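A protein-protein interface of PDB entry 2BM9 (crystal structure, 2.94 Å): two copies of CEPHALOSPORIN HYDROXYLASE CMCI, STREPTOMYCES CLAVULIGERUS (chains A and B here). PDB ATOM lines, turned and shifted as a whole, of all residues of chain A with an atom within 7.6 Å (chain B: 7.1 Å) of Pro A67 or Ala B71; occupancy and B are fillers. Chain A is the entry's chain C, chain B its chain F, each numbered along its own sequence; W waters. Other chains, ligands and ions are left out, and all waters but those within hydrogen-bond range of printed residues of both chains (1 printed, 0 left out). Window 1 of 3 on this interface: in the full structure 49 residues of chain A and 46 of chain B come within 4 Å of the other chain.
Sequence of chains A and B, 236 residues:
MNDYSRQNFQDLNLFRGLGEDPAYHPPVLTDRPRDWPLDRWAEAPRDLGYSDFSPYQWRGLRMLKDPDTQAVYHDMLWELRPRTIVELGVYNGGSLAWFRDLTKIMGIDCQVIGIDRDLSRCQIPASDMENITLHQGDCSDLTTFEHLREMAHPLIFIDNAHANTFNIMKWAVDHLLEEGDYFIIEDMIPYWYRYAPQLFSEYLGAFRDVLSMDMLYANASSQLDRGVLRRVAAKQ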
ATOM      1  N   PRO A  55      14.719  27.284 -28.936  1.00  0.00           N
ATOM      2  CA  PRO A  55      15.981  27.355 -28.198  1.00  0.00           C
ATOM      3  C   PRO A  55      16.223  26.113 -27.354  1.00  0.00           C
ATOM      4  O   PRO A  55      17.149  26.110 -26.527  1.00  0.00           O
ATOM      5  CB  PRO A  55      15.733  28.537 -27.278  1.00  0.00           C
ATOM      6  CG  PRO A  55      14.263  28.349 -26.893  1.00  0.00           C
ATOM      7  CD  PRO A  55      13.581  27.654 -28.072  1.00  0.00           C
ATOM      8  N   TYR A  56      15.405  25.081 -27.563  1.00  0.00           N
ATOM      9  CA  TYR A  56      15.439  23.889 -26.727  1.00  0.00           C
ATOM     10  C   TYR A  56      16.298  22.792 -27.342  1.00  0.00           C
ATOM     11  O   TYR A  56      16.513  22.733 -28.558  1.00  0.00           O
ATOM     12  CB  TYR A  56      14.022  23.379 -26.474  1.00  0.00           C
ATOM     13  CG  TYR A  56      13.115  24.404 -25.842  1.00  0.00           C
ATOM     14  CD1 TYR A  56      11.907  24.753 -26.437  1.00  0.00           C
ATOM     15  CD2 TYR A  56      13.469  25.015 -24.647  1.00  0.00           C
ATOM     16  CE1 TYR A  56      11.080  25.686 -25.856  1.00  0.00           C
ATOM     17  CE2 TYR A  56      12.657  25.940 -24.057  1.00  0.00           C
ATOM     18  CZ  TYR A  56      11.461  26.281 -24.657  1.00  0.00           C
ATOM     19  OH  TYR A  56      10.655  27.221 -24.050  1.00  0.00           O
ATOM     20  N   GLN A  57      16.790  21.929 -26.463  1.00  0.00           N
ATOM     21  CA  GLN A  57      17.790  20.936 -26.821  1.00  0.00           C
ATOM     22  C   GLN A  57      17.676  19.681 -25.960  1.00  0.00           C
ATOM     23  O   GLN A  57      16.811  19.593 -25.081  1.00  0.00           O
ATOM     24  CB  GLN A  57      19.195  21.539 -26.687  1.00  0.00           C
ATOM     25  CG  GLN A  57      19.658  21.769 -25.272  1.00  0.00           C
ATOM     26  CD  GLN A  57      21.126  21.489 -25.095  1.00  0.00           C
ATOM     27  OE1 GLN A  57      21.624  20.441 -25.499  1.00  0.00           O
ATOM     28  NE2 GLN A  57      21.834  22.437 -24.496  1.00  0.00           N
ATOM     29  N   MET A  63      15.815  20.261 -30.029  1.00  0.00           N
ATOM     30  CA  MET A  63      14.491  19.733 -29.721  1.00  0.00           C
ATOM     31  C   MET A  63      13.417  20.719 -30.175  1.00  0.00           C
ATOM     32  O   MET A  63      13.448  21.888 -29.794  1.00  0.00           O
ATOM     33  CB  MET A  63      14.381  19.531 -28.216  1.00  0.00           C
ATOM     34  CG  MET A  63      14.842  18.183 -27.742  1.00  0.00           C
ATOM     35  SD  MET A  63      13.659  16.940 -28.192  1.00  0.00           S
ATOM     36  CE  MET A  63      12.208  17.586 -27.449  1.00  0.00           C
ATOM     37  N   LEU A  64      12.462  20.256 -30.977  1.00  0.00           N
ATOM     38  CA  LEU A  64      11.355  21.112 -31.427  1.00  0.00           C
ATOM     39  C   LEU A  64      10.105  20.908 -30.579  1.00  0.00           C
ATOM     40  O   LEU A  64       9.166  21.690 -30.665  1.00  0.00           O
ATOM     41  CB  LEU A  64      11.021  20.860 -32.895  1.00  0.00           C
ATOM     42  CG  LEU A  64      12.188  20.665 -33.869  1.00  0.00           C
ATOM     43  CD1 LEU A  64      11.670  20.223 -35.230  1.00  0.00           C
ATOM     44  CD2 LEU A  64      13.020  21.918 -33.995  1.00  0.00           C
ATOM     45  N   LYS A  65      10.078  19.850 -29.781  1.00  0.00           N
ATOM     46  CA  LYS A  65       9.040  19.719 -28.764  1.00  0.00           C
ATOM     47  C   LYS A  65       9.449  20.637 -27.615  1.00  0.00           C
ATOM     48  O   LYS A  65      10.630  20.702 -27.277  1.00  0.00           O
ATOM     49  CB  LYS A  65       8.875  18.267 -28.286  1.00  0.00           C
ATOM     50  CG  LYS A  65       8.971  17.218 -29.403  1.00  0.00           C
ATOM     51  CD  LYS A  65       7.816  16.224 -29.377  1.00  0.00           C
ATOM     52  CE  LYS A  65       8.024  15.130 -30.422  1.00  0.00           C
ATOM     53  NZ  LYS A  65       8.187  15.662 -31.802  1.00  0.00           N
ATOM     54  N   ASP A  66       8.498  21.373 -27.040  1.00  0.00           N
ATOM     55  CA  ASP A  66       8.825  22.290 -25.954  1.00  0.00           C
ATOM     56  C   ASP A  66       8.654  21.582 -24.621  1.00  0.00           C
ATOM     57  O   ASP A  66       7.998  20.554 -24.550  1.00  0.00           O
ATOM     58  CB  ASP A  66       8.033  23.603 -26.045  1.00  0.00           C
ATOM     59  CG  ASP A  66       6.519  23.420 -26.007  1.00  0.00           C
ATOM     60  OD1 ASP A  66       5.988  22.637 -25.186  1.00  0.00           O
ATOM     61  OD2 ASP A  66       5.765  24.082 -26.760  1.00  0.00           O
ATOM     62  N   PRO A  67       9.254  22.108 -23.563  1.00  0.00           N
ATOM     63  CA  PRO A  67       9.261  21.399 -22.277  1.00  0.00           C
ATOM     64  C   PRO A  67       7.856  20.950 -21.827  1.00  0.00           C
ATOM     65  O   PRO A  67       7.707  19.919 -21.164  1.00  0.00           O
ATOM     66  CB  PRO A  67       9.839  22.439 -21.315  1.00  0.00           C
ATOM     67  CG  PRO A  67      10.628  23.354 -22.180  1.00  0.00           C
ATOM     68  CD  PRO A  67       9.945  23.408 -23.487  1.00  0.00           C
ATOM     69  N   ASP A  68       6.842  21.741 -22.180  1.00  0.00           N
ATOM     70  CA  ASP A  68       5.448  21.390 -21.943  1.00  0.00           C
ATOM     71  C   ASP A  68       5.141  20.086 -22.633  1.00  0.00           C
ATOM     72  O   ASP A  68       4.727  19.122 -22.004  1.00  0.00           O
ATOM     73  CB  ASP A  68       4.511  22.469 -22.494  1.00  0.00           C
ATOM     74  CG  ASP A  68       4.096  23.462 -21.451  1.00  0.00           C
ATOM     75  OD1 ASP A  68       3.436  24.459 -21.821  1.00  0.00           O
ATOM     76  OD2 ASP A  68       4.377  23.328 -20.238  1.00  0.00           O
ATOM     77  N   THR A  69       5.351  20.068 -23.937  1.00  0.00           N
ATOM     78  CA  THR A  69       5.121  18.885 -24.733  1.00  0.00           C
ATOM     79  C   THR A  69       5.939  17.692 -24.267  1.00  0.00           C
ATOM     80  O   THR A  69       5.452  16.581 -24.309  1.00  0.00           O
ATOM     81  CB  THR A  69       5.453  19.198 -26.154  1.00  0.00           C
ATOM     82  OG1 THR A  69       4.651  20.312 -26.579  1.00  0.00           O
ATOM     83  CG2 THR A  69       5.081  18.030 -27.065  1.00  0.00           C
ATOM     84  N   GLN A  70       7.165  17.922 -23.810  1.00  0.00           N
ATOM     85  CA  GLN A  70       8.005  16.862 -23.247  1.00  0.00           C
ATOM     86  C   GLN A  70       7.472  16.295 -21.926  1.00  0.00           C
ATOM     87  O   GLN A  70       7.758  15.159 -21.559  1.00  0.00           O
ATOM     88  CB  GLN A  70       9.413  17.384 -22.984  1.00  0.00           C
ATOM     89  CG  GLN A  70      10.199  17.843 -24.193  1.00  0.00           C
ATOM     90  CD  GLN A  70      11.471  18.577 -23.779  1.00  0.00           C
ATOM     91  OE1 GLN A  70      12.078  18.245 -22.744  1.00  0.00           O
ATOM     92  NE2 GLN A  70      11.879  19.578 -24.575  1.00  0.00           N
ATOM     93  N   ALA A  71       6.740  17.108 -21.184  1.00  0.00           N
ATOM     94  CA  ALA A  71       6.074  16.629 -19.983  1.00  0.00           C
ATOM     95  C   ALA A  71       4.889  15.735 -20.353  1.00  0.00           C
ATOM     96  O   ALA A  71       4.668  14.713 -19.709  1.00  0.00           O
ATOM     97  CB  ALA A  71       5.624  17.788 -19.121  1.00  0.00           C
ATOM     98  N   VAL A  72       4.145  16.098 -21.397  1.00  0.00           N
ATOM     99  CA  VAL A  72       3.003  15.287 -21.816  1.00  0.00           C
ATOM    100  C   VAL A  72       3.480  13.950 -22.337  1.00  0.00           C
ATOM    101  O   VAL A  72       2.839  12.929 -22.091  1.00  0.00           O
ATOM    102  CB  VAL A  72       2.151  15.931 -22.925  1.00  0.00           C
ATOM    103  CG1 VAL A  72       0.891  15.077 -23.206  1.00  0.00           C
ATOM    104  CG2 VAL A  72       1.783  17.370 -22.557  1.00  0.00           C
ATOM    105  N   TYR A  73       4.596  13.951 -23.062  1.00  0.00           N
ATOM    106  CA  TYR A  73       5.057  12.729 -23.688  1.00  0.00           C
ATOM    107  C   TYR A  73       5.647  11.842 -22.627  1.00  0.00           C
ATOM    108  O   TYR A  73       5.631  10.620 -22.748  1.00  0.00           O
ATOM    109  CB  TYR A  73       6.051  12.997 -24.810  1.00  0.00           C
ATOM    110  CG  TYR A  73       5.396  13.104 -26.165  1.00  0.00           C
ATOM    111  CD1 TYR A  73       5.638  14.191 -26.984  1.00  0.00           C
ATOM    112  CD2 TYR A  73       4.534  12.110 -26.632  1.00  0.00           C
ATOM    113  CE1 TYR A  73       5.042  14.301 -28.222  1.00  0.00           C
ATOM    114  CE2 TYR A  73       3.923  12.215 -27.880  1.00  0.00           C
ATOM    115  CZ  TYR A  73       4.176  13.317 -28.668  1.00  0.00           C
ATOM    116  OH  TYR A  73       3.583  13.426 -29.909  1.00  0.00           O
ATOM    117  N   TRP A  98      15.416  11.559 -27.854  1.00  0.00           N
ATOM    118  CA  TRP A  98      14.781  11.850 -26.590  1.00  0.00           C
ATOM    119  C   TRP A  98      13.840  10.714 -26.207  1.00  0.00           C
ATOM    120  O   TRP A  98      13.851  10.254 -25.072  1.00  0.00           O
ATOM    121  CB  TRP A  98      14.051  13.185 -26.674  1.00  0.00           C
ATOM    122  CG  TRP A  98      13.355  13.524 -25.435  1.00  0.00           C
ATOM    123  CD1 TRP A  98      13.903  14.010 -24.285  1.00  0.00           C
ATOM    124  CD2 TRP A  98      11.969  13.370 -25.184  1.00  0.00           C
ATOM    125  NE1 TRP A  98      12.932  14.179 -23.328  1.00  0.00           N
ATOM    126  CE2 TRP A  98      11.729  13.802 -23.860  1.00  0.00           C
ATOM    127  CE3 TRP A  98      10.885  12.931 -25.956  1.00  0.00           C
ATOM    128  CZ2 TRP A  98      10.462  13.790 -23.288  1.00  0.00           C
ATOM    129  CZ3 TRP A  98       9.631  12.929 -25.392  1.00  0.00           C
ATOM    130  CH2 TRP A  98       9.427  13.346 -24.064  1.00  0.00           C
ATOM    131  N   ALA A 220      -2.925  19.483 -22.671  1.00  0.00           N
ATOM    132  CA  ALA A 220      -1.850  19.830 -21.716  1.00  0.00           C
ATOM    133  C   ALA A 220      -0.573  20.296 -22.392  1.00  0.00           C
ATOM    134  O   ALA A 220       0.524  20.065 -21.880  1.00  0.00           O
ATOM    135  CB  ALA A 220      -1.531  18.625 -20.810  1.00  0.00           C
ATOM    136  N   SER A 221      -0.712  20.932 -23.547  1.00  0.00           N
ATOM    137  CA  SER A 221       0.435  21.365 -24.323  1.00  0.00           C
ATOM    138  C   SER A 221      -0.033  22.052 -25.576  1.00  0.00           C
ATOM    139  O   SER A 221      -0.810  21.462 -26.325  1.00  0.00           O
ATOM    140  CB  SER A 221       1.282  20.177 -24.746  1.00  0.00           C
ATOM    141  OG  SER A 221       2.110  20.545 -25.844  1.00  0.00           O
ATOM    142  N   GLN A 223       1.446  22.536 -28.330  1.00  0.00           N
ATOM    143  CA  GLN A 223       1.759  21.730 -29.503  1.00  0.00           C
ATOM    144  C   GLN A 223       0.815  20.550 -29.673  1.00  0.00           C
ATOM    145  O   GLN A 223       0.197  20.395 -30.718  1.00  0.00           O
ATOM    146  CB  GLN A 223       3.190  21.237 -29.448  1.00  0.00           C
ATOM    147  CG  GLN A 223       4.176  22.373 -29.557  1.00  0.00           C
ATOM    148  CD  GLN A 223       5.573  21.885 -29.687  1.00  0.00           C
ATOM    149  OE1 GLN A 223       6.052  21.156 -28.827  1.00  0.00           O
ATOM    150  NE2 GLN A 223       6.244  22.280 -30.757  1.00  0.00           N
ATOM    151  N   TYR B  56       3.340  17.486 -11.799  1.00  0.00           N
ATOM    152  CA  TYR B  56       4.463  17.110 -12.628  1.00  0.00           C
ATOM    153  C   TYR B  56       5.250  15.939 -12.048  1.00  0.00           C
ATOM    154  O   TYR B  56       5.714  15.998 -10.917  1.00  0.00           O
ATOM    155  CB  TYR B  56       5.333  18.340 -12.826  1.00  0.00           C
ATOM    156  CG  TYR B  56       4.767  19.340 -13.823  1.00  0.00           C
ATOM    157  CD1 TYR B  56       4.706  20.698 -13.520  1.00  0.00           C
ATOM    158  CD2 TYR B  56       4.307  18.924 -15.074  1.00  0.00           C
ATOM    159  CE1 TYR B  56       4.199  21.614 -14.439  1.00  0.00           C
ATOM    160  CE2 TYR B  56       3.802  19.827 -16.004  1.00  0.00           C
ATOM    161  CZ  TYR B  56       3.750  21.177 -15.690  1.00  0.00           C
ATOM    162  OH  TYR B  56       3.259  22.079 -16.624  1.00  0.00           O
ATOM    163  N   ASP B  66       8.955  22.907 -12.482  1.00  0.00           N
ATOM    164  CA  ASP B  66       8.097  22.816 -13.664  1.00  0.00           C
ATOM    165  C   ASP B  66       8.948  22.472 -14.892  1.00  0.00           C
ATOM    166  O   ASP B  66      10.185  22.468 -14.817  1.00  0.00           O
ATOM    167  CB  ASP B  66       7.188  24.061 -13.835  1.00  0.00           C
ATOM    168  CG  ASP B  66       7.947  25.388 -13.912  1.00  0.00           C
ATOM    169  OD1 ASP B  66       9.164  25.371 -14.181  1.00  0.00           O
ATOM    170  OD2 ASP B  66       7.394  26.515 -13.725  1.00  0.00           O
ATOM    171  N   PRO B  67       8.315  22.132 -16.010  1.00  0.00           N
ATOM    172  CA  PRO B  67       9.066  21.725 -17.206  1.00  0.00           C
ATOM    173  C   PRO B  67      10.134  22.743 -17.658  1.00  0.00           C
ATOM    174  O   PRO B  67      11.194  22.315 -18.115  1.00  0.00           O
ATOM    175  CB  PRO B  67       7.971  21.570 -18.267  1.00  0.00           C
ATOM    176  CG  PRO B  67       6.729  21.316 -17.493  1.00  0.00           C
ATOM    177  CD  PRO B  67       6.863  22.104 -16.244  1.00  0.00           C
ATOM    178  N   ASP B  68       9.858  24.045 -17.534  1.00  0.00           N
ATOM    179  CA  ASP B  68      10.828  25.079 -17.867  1.00  0.00           C
ATOM    180  C   ASP B  68      12.043  25.063 -16.962  1.00  0.00           C
ATOM    181  O   ASP B  68      13.165  25.182 -17.429  1.00  0.00           O
ATOM    182  CB  ASP B  68      10.184  26.433 -17.777  1.00  0.00           C
ATOM    183  CG  ASP B  68       9.189  26.662 -18.884  1.00  0.00           C
ATOM    184  OD1 ASP B  68       8.004  26.919 -18.554  1.00  0.00           O
ATOM    185  OD2 ASP B  68       9.502  26.594 -20.109  1.00  0.00           O
ATOM    186  N   THR B  69      11.835  24.912 -15.662  1.00  0.00           N
ATOM    187  CA  THR B  69      12.963  24.825 -14.755  1.00  0.00           C
ATOM    188  C   THR B  69      13.781  23.594 -15.091  1.00  0.00           C
ATOM    189  O   THR B  69      14.996  23.608 -14.947  1.00  0.00           O
ATOM    190  CB  THR B  69      12.515  24.789 -13.307  1.00  0.00           C
ATOM    191  OG1 THR B  69      12.288  26.122 -12.851  1.00  0.00           O
ATOM    192  CG2 THR B  69      13.646  24.322 -12.407  1.00  0.00           C
ATOM    193  N   GLN B  70      13.112  22.529 -15.529  1.00  0.00           N
ATOM    194  CA  GLN B  70      13.809  21.324 -15.995  1.00  0.00           C
ATOM    195  C   GLN B  70      14.630  21.668 -17.224  1.00  0.00           C
ATOM    196  O   GLN B  70      15.803  21.323 -17.317  1.00  0.00           O
ATOM    197  CB  GLN B  70      12.828  20.191 -16.318  1.00  0.00           C
ATOM    198  CG  GLN B  70      12.436  19.352 -15.109  1.00  0.00           C
ATOM    199  CD  GLN B  70      11.041  18.744 -15.230  1.00  0.00           C
ATOM    200  OE1 GLN B  70      10.539  18.542 -16.339  1.00  0.00           O
ATOM    201  NE2 GLN B  70      10.417  18.451 -14.095  1.00  0.00           N
ATOM    202  N   ALA B  71      14.023  22.386 -18.151  1.00  0.00           N
ATOM    203  CA  ALA B  71      14.728  22.775 -19.364  1.00  0.00           C
ATOM    204  C   ALA B  71      16.028  23.529 -19.064  1.00  0.00           C
ATOM    205  O   ALA B  71      17.037  23.339 -19.738  1.00  0.00           O
ATOM    206  CB  ALA B  71      13.825  23.616 -20.247  1.00  0.00           C
ATOM    207  N   VAL B  72      15.996  24.378 -18.042  1.00  0.00           N
ATOM    208  CA  VAL B  72      17.163  25.139 -17.652  1.00  0.00           C
ATOM    209  C   VAL B  72      18.183  24.171 -17.082  1.00  0.00           C
ATOM    210  O   VAL B  72      19.281  24.075 -17.602  1.00  0.00           O
ATOM    211  CB  VAL B  72      16.823  26.227 -16.629  1.00  0.00           C
ATOM    212  CG1 VAL B  72      18.073  26.878 -16.120  1.00  0.00           C
ATOM    213  CG2 VAL B  72      15.945  27.268 -17.262  1.00  0.00           C
ATOM    214  N   TYR B  73      17.813  23.421 -16.053  1.00  0.00           N
ATOM    215  CA  TYR B  73      18.772  22.559 -15.390  1.00  0.00           C
ATOM    216  C   TYR B  73      19.429  21.603 -16.376  1.00  0.00           C
ATOM    217  O   TYR B  73      20.607  21.316 -16.262  1.00  0.00           O
ATOM    218  CB  TYR B  73      18.127  21.797 -14.231  1.00  0.00           C
ATOM    219  CG  TYR B  73      18.078  22.585 -12.936  1.00  0.00           C
ATOM    220  CD1 TYR B  73      16.864  22.913 -12.349  1.00  0.00           C
ATOM    221  CD2 TYR B  73      19.246  23.023 -12.312  1.00  0.00           C
ATOM    222  CE1 TYR B  73      16.808  23.643 -11.168  1.00  0.00           C
ATOM    223  CE2 TYR B  73      19.202  23.759 -11.129  1.00  0.00           C
ATOM    224  CZ  TYR B  73      17.974  24.059 -10.554  1.00  0.00           C
ATOM    225  OH  TYR B  73      17.884  24.781  -9.381  1.00  0.00           O
ATOM    226  N   HIS B  74      18.682  21.137 -17.363  1.00  0.00           N
ATOM    227  CA  HIS B  74      19.266  20.333 -18.432  1.00  0.00           C
ATOM    228  C   HIS B  74      20.382  21.049 -19.191  1.00  0.00           C
ATOM    229  O   HIS B  74      21.462  20.501 -19.419  1.00  0.00           O
ATOM    230  CB  HIS B  74      18.221  19.956 -19.470  1.00  0.00           C
ATOM    231  CG  HIS B  74      18.822  19.407 -20.724  1.00  0.00           C
ATOM    232  ND1 HIS B  74      18.985  20.157 -21.869  1.00  0.00           N
ATOM    233  CD2 HIS B  74      19.352  18.191 -20.990  1.00  0.00           C
ATOM    234  CE1 HIS B  74      19.572  19.414 -22.792  1.00  0.00           C
ATOM    235  NE2 HIS B  74      19.801  18.217 -22.286  1.00  0.00           N
ATOM    236  N   ASP B  75      20.093  22.256 -19.644  1.00  0.00           N
ATOM    237  CA  ASP B  75      21.088  23.012 -20.375  1.00  0.00           C
ATOM    238  C   ASP B  75      22.324  23.186 -19.483  1.00  0.00           C
ATOM    239  O   ASP B  75      23.426  22.829 -19.879  1.00  0.00           O
ATOM    240  CB  ASP B  75      20.514  24.358 -20.845  1.00  0.00           C
ATOM    241  CG  ASP B  75      19.337  24.202 -21.831  1.00  0.00           C
ATOM    242  OD1 ASP B  75      19.158  23.106 -22.406  1.00  0.00           O
ATOM    243  OD2 ASP B  75      18.538  25.132 -22.088  1.00  0.00           O
ATOM    244  N   MET B  76      22.119  23.675 -18.264  1.00  0.00           N
ATOM    245  CA  MET B  76      23.202  23.957 -17.317  1.00  0.00           C
ATOM    246  C   MET B  76      24.074  22.752 -17.050  1.00  0.00           C
ATOM    247  O   MET B  76      25.282  22.879 -16.911  1.00  0.00           O
ATOM    248  CB  MET B  76      22.619  24.432 -15.980  1.00  0.00           C
ATOM    249  CG  MET B  76      23.665  24.886 -14.954  1.00  0.00           C
ATOM    250  SD  MET B  76      22.957  25.295 -13.346  1.00  0.00           S
ATOM    251  CE  MET B  76      21.653  26.363 -13.852  1.00  0.00           C
ATOM    252  N   TRP B  98      15.774  12.837 -10.456  1.00  0.00           N
ATOM    253  CA  TRP B  98      15.850  13.435 -11.778  1.00  0.00           C
ATOM    254  C   TRP B  98      17.304  13.753 -12.088  1.00  0.00           C
ATOM    255  O   TRP B  98      17.842  13.337 -13.115  1.00  0.00           O
ATOM    256  CB  TRP B  98      15.013  14.702 -11.833  1.00  0.00           C
ATOM    257  CG  TRP B  98      14.930  15.264 -13.203  1.00  0.00           C
ATOM    258  CD1 TRP B  98      14.317  14.697 -14.284  1.00  0.00           C
ATOM    259  CD2 TRP B  98      15.487  16.496 -13.661  1.00  0.00           C
ATOM    260  NE1 TRP B  98      14.451  15.508 -15.386  1.00  0.00           N
ATOM    261  CE2 TRP B  98      15.164  16.622 -15.033  1.00  0.00           C
ATOM    262  CE3 TRP B  98      16.220  17.517 -13.051  1.00  0.00           C
ATOM    263  CZ2 TRP B  98      15.548  17.723 -15.799  1.00  0.00           C
ATOM    264  CZ3 TRP B  98      16.603  18.604 -13.810  1.00  0.00           C
ATOM    265  CH2 TRP B  98      16.270  18.695 -15.176  1.00  0.00           C
ATOM    266  N   TYR B 217      20.919  31.671 -17.933  1.00  0.00           N
ATOM    267  CA  TYR B 217      19.840  30.894 -17.329  1.00  0.00           C
ATOM    268  C   TYR B 217      18.852  31.679 -16.480  1.00  0.00           C
ATOM    269  O   TYR B 217      17.757  31.202 -16.214  1.00  0.00           O
ATOM    270  CB  TYR B 217      20.433  29.773 -16.485  1.00  0.00           C
ATOM    271  CG  TYR B 217      21.326  28.889 -17.302  1.00  0.00           C
ATOM    272  CD1 TYR B 217      22.652  28.679 -16.950  1.00  0.00           C
ATOM    273  CD2 TYR B 217      20.850  28.284 -18.459  1.00  0.00           C
ATOM    274  CE1 TYR B 217      23.468  27.876 -17.729  1.00  0.00           C
ATOM    275  CE2 TYR B 217      21.648  27.482 -19.230  1.00  0.00           C
ATOM    276  CZ  TYR B 217      22.951  27.278 -18.870  1.00  0.00           C
ATOM    277  OH  TYR B 217      23.730  26.466 -19.656  1.00  0.00           O
ATOM    278  N   ALA B 220      15.124  32.459 -17.547  1.00  0.00           N
ATOM    279  CA  ALA B 220      14.586  31.411 -18.410  1.00  0.00           C
ATOM    280  C   ALA B 220      13.542  30.509 -17.739  1.00  0.00           C
ATOM    281  O   ALA B 220      13.081  29.551 -18.368  1.00  0.00           O
ATOM    282  CB  ALA B 220      15.729  30.561 -18.978  1.00  0.00           C
ATOM    283  N   SER B 221      13.168  30.783 -16.488  1.00  0.00           N
ATOM    284  CA  SER B 221      12.077  30.030 -15.851  1.00  0.00           C
ATOM    285  C   SER B 221      11.491  30.728 -14.631  1.00  0.00           C
ATOM    286  O   SER B 221      12.218  31.360 -13.876  1.00  0.00           O
ATOM    287  CB  SER B 221      12.547  28.635 -15.452  1.00  0.00           C
ATOM    288  OG  SER B 221      13.028  28.621 -14.117  1.00  0.00           O
ATOM    289  N   LEU B 224      13.444  29.756 -11.308  1.00  0.00           N
ATOM    290  CA  LEU B 224      14.821  30.212 -11.200  1.00  0.00           C
ATOM    291  C   LEU B 224      14.946  31.723 -11.392  1.00  0.00           C
ATOM    292  O   LEU B 224      16.030  32.261 -11.258  1.00  0.00           O
ATOM    293  CB  LEU B 224      15.703  29.498 -12.221  1.00  0.00           C
ATOM    294  CG  LEU B 224      15.629  27.977 -12.210  1.00  0.00           C
ATOM    295  CD1 LEU B 224      16.188  27.437 -13.503  1.00  0.00           C
ATOM    296  CD2 LEU B 224      16.382  27.400 -11.001  1.00  0.00           C
HETATM  297  O   HOH W   1      16.046  22.027 -23.157  1.00  0.00           O
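Pro B67 touches its own counterpart, Pro A67.
Pro A67 touches Ala B71, but with the chains exchanged Ala A71 does not touch Pro B67 (4.04 Å).
Asp A68 touches Tyr B56, but with the chains exchanged Tyr A56 does not touch Asp B68 (4.2 Å).
Of the 5 pairs that touch across the chains among the printed residues, 1 has its exchanged pair printed and touching as well.
OD1 of Asp A66 sits close to N of Asp A68 (3.3 Å).
The side-chain carboxylate of Asp B75 sits at hydrogen-bond distance from a ring nitrogen (ND1) of His B74, 3.0 Å away.
Water W1 bridges the backbone carbonyl oxygen (O) of Gln A57 and the side-chain carboxylate (OD1) of Asp B75.
The side-chain amide nitrogen (NE2) of Gln A57 lies close to the side-chain carboxylate (OD1) of Asp B75, 3.5 Å away.
Of the printed residues of chain B, Pro A67 touches Pro B67 and Ala B71.
Ala B71 touches just one residue of chain A: Pro A67.
Of the printed residues of chain B, Asp A68 touches Tyr B56.
Printed residues of chain A within 4 Å of Asp B75: Gln A57 (3.2 Å).
Printed residues of chain A within 4 Å of Pro B67: Pro A67.
The nearest printed residue of chain B that does not touch Pro A67 is Asp B68 (4.01 Å).
The nearest residue of chain A that does not touch Ala B71 is Tyr A56 (4.6 Å).
Printed residues of chain A that touch a printed residue of chain B: Gln A57, Pro A67 and Asp A68.
Hydrophobic or aromatic side chains of chain A that line the printed part of chain B: Pro A67.
Of the 17 printed residues of chain B, 5 touch a printed residue of chain A.
Printed residues of chain B that touch a printed residue of chain A: Tyr B56, Pro B67, Ala B71, His B74 and Asp B75.
Among the printed residues, 5 pairs touch across the chains.
CG of Gln A57 touches CE1 of His B74, 3.4 Å away.
Pro A67 touches Pro B67 (O to CB, 3.3 Å).
Pro A67 touches Ala B71 (CG to CB, 3.7 Å).
Tyr B56 touches Asp A68 (OH to OD2, 3.98 Å).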
